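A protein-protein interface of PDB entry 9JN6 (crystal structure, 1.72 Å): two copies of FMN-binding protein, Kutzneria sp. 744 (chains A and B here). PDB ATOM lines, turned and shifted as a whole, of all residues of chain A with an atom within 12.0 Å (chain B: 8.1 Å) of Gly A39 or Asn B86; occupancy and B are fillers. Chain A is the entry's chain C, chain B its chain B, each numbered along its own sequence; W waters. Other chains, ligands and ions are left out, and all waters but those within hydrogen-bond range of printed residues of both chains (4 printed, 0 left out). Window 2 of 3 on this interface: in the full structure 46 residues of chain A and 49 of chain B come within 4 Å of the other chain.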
ATOM      1  N   ALA A  33      29.901  15.567 -32.507  1.00  0.00           N
ATOM      2  CA  ALA A  33      29.231  15.673 -31.198  1.00  0.00           C
ATOM      3  C   ALA A  33      27.807  15.110 -31.277  1.00  0.00           C
ATOM      4  O   ALA A  33      27.049  15.512 -32.171  1.00  0.00           O
ATOM      5  CB  ALA A  33      29.230  17.101 -30.685  1.00  0.00           C
ATOM      6  N   SER A  34      27.417  14.408 -30.223  1.00  0.00           N
ATOM      7  CA  SER A  34      26.013  14.022 -29.989  1.00  0.00           C
ATOM      8  C   SER A  34      25.637  14.143 -28.512  1.00  0.00           C
ATOM      9  O   SER A  34      26.507  14.245 -27.663  1.00  0.00           O
ATOM     10  CB  SER A  34      25.731  12.660 -30.537  1.00  0.00           C
ATOM     11  OG  SER A  34      26.456  11.700 -29.814  1.00  0.00           O
ATOM     12  N   ASN A  35      24.344  14.239 -28.239  1.00  0.00           N
ATOM     13  CA  ASN A  35      23.866  14.507 -26.862  1.00  0.00           C
ATOM     14  C   ASN A  35      24.255  13.385 -25.901  1.00  0.00           C
ATOM     15  O   ASN A  35      24.237  12.161 -26.292  1.00  0.00           O
ATOM     16  CB  ASN A  35      22.362  14.747 -26.807  1.00  0.00           C
ATOM     17  CG  ASN A  35      21.934  16.060 -27.414  1.00  0.00           C
ATOM     18  OD1 ASN A  35      22.714  16.991 -27.566  1.00  0.00           O
ATOM     19  ND2 ASN A  35      20.660  16.140 -27.783  1.00  0.00           N
ATOM     20  N   GLY A  36      24.583  13.785 -24.661  1.00  0.00           N
ATOM     21  CA  GLY A  36      24.885  12.849 -23.573  1.00  0.00           C
ATOM     22  C   GLY A  36      23.550  12.414 -22.975  1.00  0.00           C
ATOM     23  O   GLY A  36      22.639  13.239 -22.943  1.00  0.00           O
ATOM     24  N   ALA A  37      23.414  11.158 -22.608  1.00  0.00           N
ATOM     25  CA  ALA A  37      22.160  10.603 -22.052  1.00  0.00           C
ATOM     26  C   ALA A  37      22.019  11.133 -20.629  1.00  0.00           C
ATOM     27  O   ALA A  37      23.075  11.275 -19.955  1.00  0.00           O
ATOM     28  CB  ALA A  37      22.195   9.104 -22.099  1.00  0.00           C
ATOM     29  N   GLY A  38      20.780  11.471 -20.241  1.00  0.00           N
ATOM     30  CA  GLY A  38      20.407  11.825 -18.860  1.00  0.00           C
ATOM     31  C   GLY A  38      21.042  13.136 -18.449  1.00  0.00           C
ATOM     32  O   GLY A  38      21.519  13.211 -17.331  1.00  0.00           O
ATOM     33  N   GLY A  39      21.026  14.122 -19.348  1.00  0.00           N
ATOM     34  CA  GLY A  39      21.608  15.464 -19.152  1.00  0.00           C
ATOM     35  C   GLY A  39      23.119  15.456 -18.951  1.00  0.00           C
ATOM     36  O   GLY A  39      23.652  16.506 -18.533  1.00  0.00           O
ATOM     37  N   ALA A  40      23.809  14.363 -19.258  1.00  0.00           N
ATOM     38  CA  ALA A  40      25.288  14.316 -19.242  1.00  0.00           C
ATOM     39  C   ALA A  40      25.828  15.167 -20.408  1.00  0.00           C
ATOM     40  O   ALA A  40      25.074  15.519 -21.330  1.00  0.00           O
ATOM     41  CB  ALA A  40      25.812  12.897 -19.253  1.00  0.00           C
ATOM     42  N   ALA A  41      27.071  15.616 -20.304  1.00  0.00           N
ATOM     43  CA  ALA A  41      27.731  16.395 -21.371  1.00  0.00           C
ATOM     44  C   ALA A  41      27.698  15.579 -22.668  1.00  0.00           C
ATOM     45  O   ALA A  41      27.784  14.351 -22.659  1.00  0.00           O
ATOM     46  CB  ALA A  41      29.146  16.684 -20.960  1.00  0.00           C
ATOM     47  N   PRO A  42      27.703  16.251 -23.827  1.00  0.00           N
ATOM     48  CA  PRO A  42      27.874  15.561 -25.090  1.00  0.00           C
ATOM     49  C   PRO A  42      29.064  14.600 -25.174  1.00  0.00           C
ATOM     50  O   PRO A  42      30.060  14.801 -24.522  1.00  0.00           O
ATOM     51  CB  PRO A  42      28.045  16.688 -26.093  1.00  0.00           C
ATOM     52  CG  PRO A  42      27.239  17.828 -25.505  1.00  0.00           C
ATOM     53  CD  PRO A  42      27.453  17.685 -24.014  1.00  0.00           C
ATOM     54  N   HIS A  43      28.897  13.565 -26.017  1.00  0.00           N
ATOM     55  CA  HIS A  43      29.975  12.704 -26.564  1.00  0.00           C
ATOM     56  C   HIS A  43      30.664  13.469 -27.705  1.00  0.00           C
ATOM     57  O   HIS A  43      29.949  14.137 -28.475  1.00  0.00           O
ATOM     58  CB  HIS A  43      29.422  11.417 -27.148  1.00  0.00           C
ATOM     59  CG  HIS A  43      28.616  10.640 -26.167  1.00  0.00           C
ATOM     60  ND1 HIS A  43      29.210   9.819 -25.253  1.00  0.00           N
ATOM     61  CD2 HIS A  43      27.286  10.542 -25.975  1.00  0.00           C
ATOM     62  CE1 HIS A  43      28.283   9.226 -24.525  1.00  0.00           C
ATOM     63  NE2 HIS A  43      27.095   9.659 -24.939  1.00  0.00           N
ATOM     64  N   ILE A  44      31.985  13.453 -27.723  1.00  0.00           N
ATOM     65  CA  ILE A  44      32.874  14.125 -28.720  1.00  0.00           C
ATOM     66  C   ILE A  44      33.880  13.111 -29.220  1.00  0.00           C
ATOM     67  O   ILE A  44      34.638  12.605 -28.383  1.00  0.00           O
ATOM     68  CB  ILE A  44      33.642  15.311 -28.100  1.00  0.00           C
ATOM     69  CG1 ILE A  44      32.744  16.287 -27.366  1.00  0.00           C
ATOM     70  CG2 ILE A  44      34.470  16.017 -29.137  1.00  0.00           C
ATOM     71  CD1 ILE A  44      31.757  16.990 -28.217  1.00  0.00           C
ATOM     72  N   ALA A  80      26.191   4.955 -28.459  1.00  0.00           N
ATOM     73  CA  ALA A  80      25.392   6.042 -27.905  1.00  0.00           C
ATOM     74  C   ALA A  80      24.651   6.698 -29.066  1.00  0.00           C
ATOM     75  O   ALA A  80      23.585   7.270 -28.847  1.00  0.00           O
ATOM     76  CB  ALA A  80      26.277   6.996 -27.143  1.00  0.00           C
ATOM     77  N   LEU B  32      33.252  24.514 -26.796  1.00  0.00           N
ATOM     78  CA  LEU B  32      32.372  24.239 -25.644  1.00  0.00           C
ATOM     79  C   LEU B  32      31.088  23.599 -26.187  1.00  0.00           C
ATOM     80  O   LEU B  32      30.456  24.234 -26.980  1.00  0.00           O
ATOM     81  CB  LEU B  32      32.064  25.569 -24.958  1.00  0.00           C
ATOM     82  CG  LEU B  32      31.100  25.457 -23.779  1.00  0.00           C
ATOM     83  CD1 LEU B  32      31.738  24.701 -22.649  1.00  0.00           C
ATOM     84  CD2 LEU B  32      30.609  26.823 -23.334  1.00  0.00           C
ATOM     85  N   ALA B  33      30.726  22.428 -25.696  1.00  0.00           N
ATOM     86  CA  ALA B  33      29.564  21.651 -26.134  1.00  0.00           C
ATOM     87  C   ALA B  33      28.619  21.385 -24.948  1.00  0.00           C
ATOM     88  O   ALA B  33      29.070  20.957 -23.883  1.00  0.00           O
ATOM     89  CB  ALA B  33      29.996  20.375 -26.817  1.00  0.00           C
ATOM     90  N   SER B  34      27.346  21.618 -25.192  1.00  0.00           N
ATOM     91  CA  SER B  34      26.241  21.184 -24.321  1.00  0.00           C
ATOM     92  C   SER B  34      25.094  20.609 -25.147  1.00  0.00           C
ATOM     93  O   SER B  34      25.008  20.856 -26.340  1.00  0.00           O
ATOM     94  CB  SER B  34      25.791  22.321 -23.470  1.00  0.00           C
ATOM     95  OG  SER B  34      25.271  23.401 -24.231  1.00  0.00           O
ATOM     96  N   ASN B  35      24.196  19.901 -24.490  1.00  0.00           N
ATOM     97  CA  ASN B  35      23.122  19.146 -25.167  1.00  0.00           C
ATOM     98  C   ASN B  35      22.168  20.115 -25.860  1.00  0.00           C
ATOM     99  O   ASN B  35      21.867  21.172 -25.273  1.00  0.00           O
ATOM    100  CB  ASN B  35      22.365  18.241 -24.208  1.00  0.00           C
ATOM    101  CG  ASN B  35      23.165  17.056 -23.748  1.00  0.00           C
ATOM    102  OD1 ASN B  35      24.154  16.700 -24.373  1.00  0.00           O
ATOM    103  ND2 ASN B  35      22.647  16.362 -22.744  1.00  0.00           N
ATOM    104  N   HIS B  77      23.453  30.111 -27.284  1.00  0.00           N
ATOM    105  CA  HIS B  77      24.069  29.064 -26.457  1.00  0.00           C
ATOM    106  C   HIS B  77      24.108  29.538 -24.992  1.00  0.00           C
ATOM    107  O   HIS B  77      23.891  28.718 -24.065  1.00  0.00           O
ATOM    108  CB  HIS B  77      25.444  28.753 -27.050  1.00  0.00           C
ATOM    109  CG  HIS B  77      26.063  27.545 -26.466  1.00  0.00           C
ATOM    110  ND1 HIS B  77      27.311  27.069 -26.884  1.00  0.00           N
ATOM    111  CD2 HIS B  77      25.612  26.673 -25.551  1.00  0.00           C
ATOM    112  CE1 HIS B  77      27.579  25.968 -26.227  1.00  0.00           C
ATOM    113  NE2 HIS B  77      26.547  25.689 -25.444  1.00  0.00           N
ATOM    114  N   LEU B  81      22.357  27.404 -21.821  1.00  0.00           N
ATOM    115  CA  LEU B  81      23.121  26.753 -20.729  1.00  0.00           C
ATOM    116  C   LEU B  81      22.296  26.793 -19.428  1.00  0.00           C
ATOM    117  O   LEU B  81      22.530  25.940 -18.523  1.00  0.00           O
ATOM    118  CB  LEU B  81      24.474  27.462 -20.591  1.00  0.00           C
ATOM    119  CG  LEU B  81      25.467  27.058 -21.675  1.00  0.00           C
ATOM    120  CD1 LEU B  81      26.565  28.064 -21.796  1.00  0.00           C
ATOM    121  CD2 LEU B  81      26.023  25.670 -21.421  1.00  0.00           C
ATOM    122  N   GLY B  83      21.037  26.976 -15.919  1.00  0.00           N
ATOM    123  CA  GLY B  83      21.647  26.923 -14.575  1.00  0.00           C
ATOM    124  C   GLY B  83      22.971  26.179 -14.565  1.00  0.00           C
ATOM    125  O   GLY B  83      23.986  26.752 -14.996  1.00  0.00           O
ATOM    126  N   ALA B  84      22.956  24.937 -14.085  1.00  0.00           N
ATOM    127  CA  ALA B  84      24.154  24.104 -13.844  1.00  0.00           C
ATOM    128  C   ALA B  84      24.318  23.100 -14.997  1.00  0.00           C
ATOM    129  O   ALA B  84      24.182  21.877 -14.746  1.00  0.00           O
ATOM    130  CB  ALA B  84      24.009  23.405 -12.512  1.00  0.00           C
ATOM    131  N   ALA B  85      24.618  23.584 -16.208  1.00  0.00           N
ATOM    132  CA  ALA B  85      24.696  22.735 -17.424  1.00  0.00           C
ATOM    133  C   ALA B  85      25.940  21.844 -17.339  1.00  0.00           C
ATOM    134  O   ALA B  85      27.009  22.352 -17.015  1.00  0.00           O
ATOM    135  CB  ALA B  85      24.704  23.579 -18.663  1.00  0.00           C
ATOM    136  N   ASN B  86      25.778  20.559 -17.634  1.00  0.00           N
ATOM    137  CA  ASN B  86      26.906  19.623 -17.764  1.00  0.00           C
ATOM    138  C   ASN B  86      27.472  19.840 -19.157  1.00  0.00           C
ATOM    139  O   ASN B  86      26.703  19.803 -20.116  1.00  0.00           O
ATOM    140  CB  ASN B  86      26.462  18.184 -17.585  1.00  0.00           C
ATOM    141  CG  ASN B  86      26.010  17.982 -16.169  1.00  0.00           C
ATOM    142  OD1 ASN B  86      26.651  18.515 -15.267  1.00  0.00           O
ATOM    143  ND2 ASN B  86      24.908  17.280 -15.982  1.00  0.00           N
ATOM    144  N   VAL B  87      28.746  20.176 -19.237  1.00  0.00           N
ATOM    145  CA  VAL B  87      29.362  20.571 -20.535  1.00  0.00           C
ATOM    146  C   VAL B  87      30.635  19.781 -20.742  1.00  0.00           C
ATOM    147  O   VAL B  87      31.181  19.264 -19.806  1.00  0.00           O
ATOM    148  CB  VAL B  87      29.659  22.073 -20.620  1.00  0.00           C
ATOM    149  CG1 VAL B  87      28.390  22.909 -20.457  1.00  0.00           C
ATOM    150  CG2 VAL B  87      30.770  22.506 -19.688  1.00  0.00           C
ATOM    151  N   VAL B  88      31.098  19.785 -21.989  1.00  0.00           N
ATOM    152  CA  VAL B  88      32.462  19.327 -22.356  1.00  0.00           C
ATOM    153  C   VAL B  88      33.147  20.500 -23.067  1.00  0.00           C
ATOM    154  O   VAL B  88      32.435  21.285 -23.787  1.00  0.00           O
ATOM    155  CB  VAL B  88      32.475  18.036 -23.203  1.00  0.00           C
ATOM    156  CG1 VAL B  88      31.624  18.175 -24.439  1.00  0.00           C
ATOM    157  CG2 VAL B  88      33.908  17.683 -23.599  1.00  0.00           C
ATOM    158  N   ALA B  89      34.398  20.754 -22.721  1.00  0.00           N
ATOM    159  CA  ALA B  89      35.247  21.739 -23.463  1.00  0.00           C
ATOM    160  C   ALA B  89      36.413  20.983 -24.038  1.00  0.00           C
ATOM    161  O   ALA B  89      37.088  20.231 -23.289  1.00  0.00           O
ATOM    162  CB  ALA B  89      35.637  22.920 -22.610  1.00  0.00           C
ATOM    163  N   VAL B 119      37.571  18.268 -21.261  1.00  0.00           N
ATOM    164  CA  VAL B 119      37.266  18.441 -19.832  1.00  0.00           C
ATOM    165  C   VAL B 119      35.752  18.453 -19.699  1.00  0.00           C
ATOM    166  O   VAL B 119      35.054  19.115 -20.510  1.00  0.00           O
ATOM    167  CB  VAL B 119      37.928  19.676 -19.192  1.00  0.00           C
ATOM    168  CG1 VAL B 119      39.442  19.584 -19.237  1.00  0.00           C
ATOM    169  CG2 VAL B 119      37.433  20.995 -19.773  1.00  0.00           C
ATOM    170  N   ARG B 120      35.264  17.830 -18.653  1.00  0.00           N
ATOM    171  CA  ARG B 120      33.814  17.756 -18.369  1.00  0.00           C
ATOM    172  C   ARG B 120      33.538  18.283 -16.976  1.00  0.00           C
ATOM    173  O   ARG B 120      34.319  18.035 -16.086  1.00  0.00           O
ATOM    174  CB  ARG B 120      33.325  16.330 -18.576  1.00  0.00           C
ATOM    175  CG  ARG B 120      33.207  15.968 -20.047  1.00  0.00           C
ATOM    176  CD  ARG B 120      32.787  14.527 -20.249  1.00  0.00           C
ATOM    177  NE  ARG B 120      32.392  14.339 -21.641  1.00  0.00           N
ATOM    178  CZ  ARG B 120      33.224  14.193 -22.667  1.00  0.00           C
ATOM    179  NH1 ARG B 120      34.533  14.173 -22.499  1.00  0.00           N
ATOM    180  NH2 ARG B 120      32.732  14.068 -23.875  1.00  0.00           N
ATOM    181  N   GLY B 121      32.514  19.095 -16.841  1.00  0.00           N
ATOM    182  CA  GLY B 121      31.978  19.418 -15.507  1.00  0.00           C
ATOM    183  C   GLY B 121      30.833  20.373 -15.652  1.00  0.00           C
ATOM    184  O   GLY B 121      30.292  20.468 -16.766  1.00  0.00           O
ATOM    185  N   GLU B 122      30.451  21.017 -14.566  1.00  0.00           N
ATOM    186  CA  GLU B 122      29.251  21.883 -14.517  1.00  0.00           C
ATOM    187  C   GLU B 122      29.687  23.318 -14.796  1.00  0.00           C
ATOM    188  O   GLU B 122      30.603  23.811 -14.132  1.00  0.00           O
ATOM    189  CB  GLU B 122      28.581  21.624 -13.166  1.00  0.00           C
ATOM    190  CG  GLU B 122      27.331  22.409 -12.897  1.00  0.00           C
ATOM    191  CD  GLU B 122      26.906  22.229 -11.438  1.00  0.00           C
ATOM    192  OE1 GLU B 122      26.974  23.228 -10.685  1.00  0.00           O
ATOM    193  OE2 GLU B 122      26.545  21.077 -11.051  1.00  0.00           O
ATOM    194  N   LEU B 123      29.124  23.936 -15.828  1.00  0.00           N
ATOM    195  CA  LEU B 123      29.411  25.339 -16.135  1.00  0.00           C
ATOM    196  C   LEU B 123      28.516  26.168 -15.235  1.00  0.00           C
ATOM    197  O   LEU B 123      27.318  25.864 -15.161  1.00  0.00           O
ATOM    198  CB  LEU B 123      29.133  25.603 -17.602  1.00  0.00           C
ATOM    199  CG  LEU B 123      29.438  27.012 -18.124  1.00  0.00           C
ATOM    200  CD1 LEU B 123      29.836  26.943 -19.586  1.00  0.00           C
ATOM    201  CD2 LEU B 123      28.254  27.971 -17.984  1.00  0.00           C
ATOM    202  N   ARG B 124      29.105  27.096 -14.490  1.00  0.00           N
ATOM    203  CA  ARG B 124      28.316  28.066 -13.710  1.00  0.00           C
ATOM    204  C   ARG B 124      28.574  29.440 -14.270  1.00  0.00           C
ATOM    205  O   ARG B 124      29.743  29.806 -14.461  1.00  0.00           O
ATOM    206  CB  ARG B 124      28.581  27.935 -12.210  1.00  0.00           C
ATOM    207  CG  ARG B 124      30.033  27.864 -11.801  1.00  0.00           C
ATOM    208  CD  ARG B 124      30.099  27.795 -10.283  1.00  0.00           C
ATOM    209  NE  ARG B 124      31.362  28.300  -9.779  1.00  0.00           N
ATOM    210  CZ  ARG B 124      31.656  29.585  -9.635  1.00  0.00           C
ATOM    211  NH1 ARG B 124      30.779  30.523  -9.981  1.00  0.00           N
ATOM    212  NH2 ARG B 124      32.845  29.914  -9.153  1.00  0.00           N
ATOM    213  N   LEU B 172      34.205  26.721 -14.891  1.00  0.00           N
ATOM    214  CA  LEU B 172      33.967  25.310 -15.172  1.00  0.00           C
ATOM    215  C   LEU B 172      34.871  24.525 -14.241  1.00  0.00           C
ATOM    216  O   LEU B 172      36.057  24.537 -14.468  1.00  0.00           O
ATOM    217  CB  LEU B 172      34.268  25.035 -16.647  1.00  0.00           C
ATOM    218  CG  LEU B 172      34.133  23.590 -17.111  1.00  0.00           C
ATOM    219  CD1 LEU B 172      32.742  22.985 -16.790  1.00  0.00           C
ATOM    220  CD2 LEU B 172      34.393  23.539 -18.608  1.00  0.00           C
ATOM    221  N   ALA B 175      35.495  18.055 -13.443  1.00  0.00           N
ATOM    222  CA  ALA B 175      35.158  16.764 -12.794  1.00  0.00           C
ATOM    223  C   ALA B 175      35.944  15.624 -13.433  1.00  0.00           C
ATOM    224  O   ALA B 175      36.301  14.663 -12.741  1.00  0.00           O
ATOM    225  CB  ALA B 175      33.683  16.493 -12.920  1.00  0.00           C
HETATM  226  O   HOH W   1      33.619  11.886 -25.762  1.00  0.00           O
HETATM  227  O   HOH W   2      23.045  19.554 -18.328  1.00  0.00           O
HETATM  228  O   HOH W   3      29.792  13.088 -21.719  1.00  0.00           O
HETATM  229  O   HOH W   4      24.744  18.906 -21.696  1.00  0.00           O
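OD1 of Asn B35 lies within hydrogen-bond range of N of Gly A36, at 3.0 Å.
O of Ala A40 is in hydrogen-bond range of ND2 of Asn B35, at 2.9 Å.
ND2 of Asn B86 is in hydrogen-bond range of O of Gly A39 (2.9 Å).
NH2 of Arg B120 lies within hydrogen-bond range of O of Pro A42, 2.8 Å away.
The backbone carbonyl oxygen (O) of Val B88 sits at hydrogen-bond distance from the backbone NH (N) of Ala B33, at 2.8 Å.
The side-chain hydroxyl (OG) of Ser B34 is in hydrogen-bond range of a ring nitrogen (NE2) of His B77 (2.9 Å).
N of Val B87 is in hydrogen-bond range of O of Gly B121, at 2.9 Å.
N of Ala B175 is in hydrogen-bond range of O of Arg B120.
Among the printed residues, merely in contact across the chains: Asn A35 with Asn B35, Gly A39 with Asn B35, Ala A41 with Asn B86, Ala A41 with Val B87, Ala A41 with Val B88, Pro A42 with Ala B33, Pro A42 with Ser B34, Pro A42 with Asn B35, Pro A42 with Val B88, Ile A44 with Val B88 and Ile A44 with Arg B120.
Of the printed residues of chain B, Gly A39 touches Asn B35 and Asn B86.
Of chain A, only Gly A39 and Ala A41 come within 4 Å of Asn B86.
No residue of chain B comes within 4 Å of Gly A38.
Ala A40 touches just one residue of chain B: Asn B35.
Ala B33 touches one residue of chain A.
Of chain A, only Asn A35, Gly A36, Gly A39, Ala A40 and Pro A42 come within 4 Å of Asn B35.
Val B87 touches one residue of chain A.
No residue of chain A comes within 4 Å of Glu B122.
Leu B123 touches none of the printed residues of chain A.
Of the printed residues of chain B, Asn A35 touches Asn B35.
Printed residues of chain B within 4 Å of Gly A36: Asn B35.
Printed residues of chain B within 4 Å of Ala A41: Asn B86, Val B87 and Val B88.
Of the printed residues of chain A, Val B88 touches Ala A41, Pro A42 and Ile A44.
Of the printed residues of chain B, Pro A42 touches Ala B33 (3.7 Å), Ser B34 (3.5 Å), Asn B35 (3.5 Å), Val B88 (3.7 Å) and Arg B120 (2.8 Å).
The nearest residue of chain B that does not touch Gly A39 is Ala B85 (5.9 Å).
Hydrophobic or aromatic side chains of chain A that line the printed part of chain B: Ala A41, Pro A42 and Ile A44.
Hydrophobic or aromatic side chains of chain B within 4 Å of the printed part of chain A: Ala B33 and Val B88.
Asn A35 touches its own counterpart, Asn B35.
3 positions are printed for both chains.
Of the 15 pairs that touch across the chains among the printed residues, 1 has its exchanged pair printed and touching as well.
Water W3 lies within hydrogen-bond range of the backbone carbonyl oxygen (O) of Ala A41, the guanidinium group (NE) of Arg B120 and the backbone carbonyl oxygen (O) of Pro A42.
Water W4 lies within hydrogen-bond range of the backbone carbonyl oxygen of Asn B86, the backbone NH of Asn B35 and the backbone carbonyl oxygen of Ala A40.
Water W1 lies within hydrogen-bond range of O of Ile A44 and NH2 of Arg B120.
Water W2 bridges N of Asn B86 (3.0 Å) and O of Gly A39 (3.1 Å).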
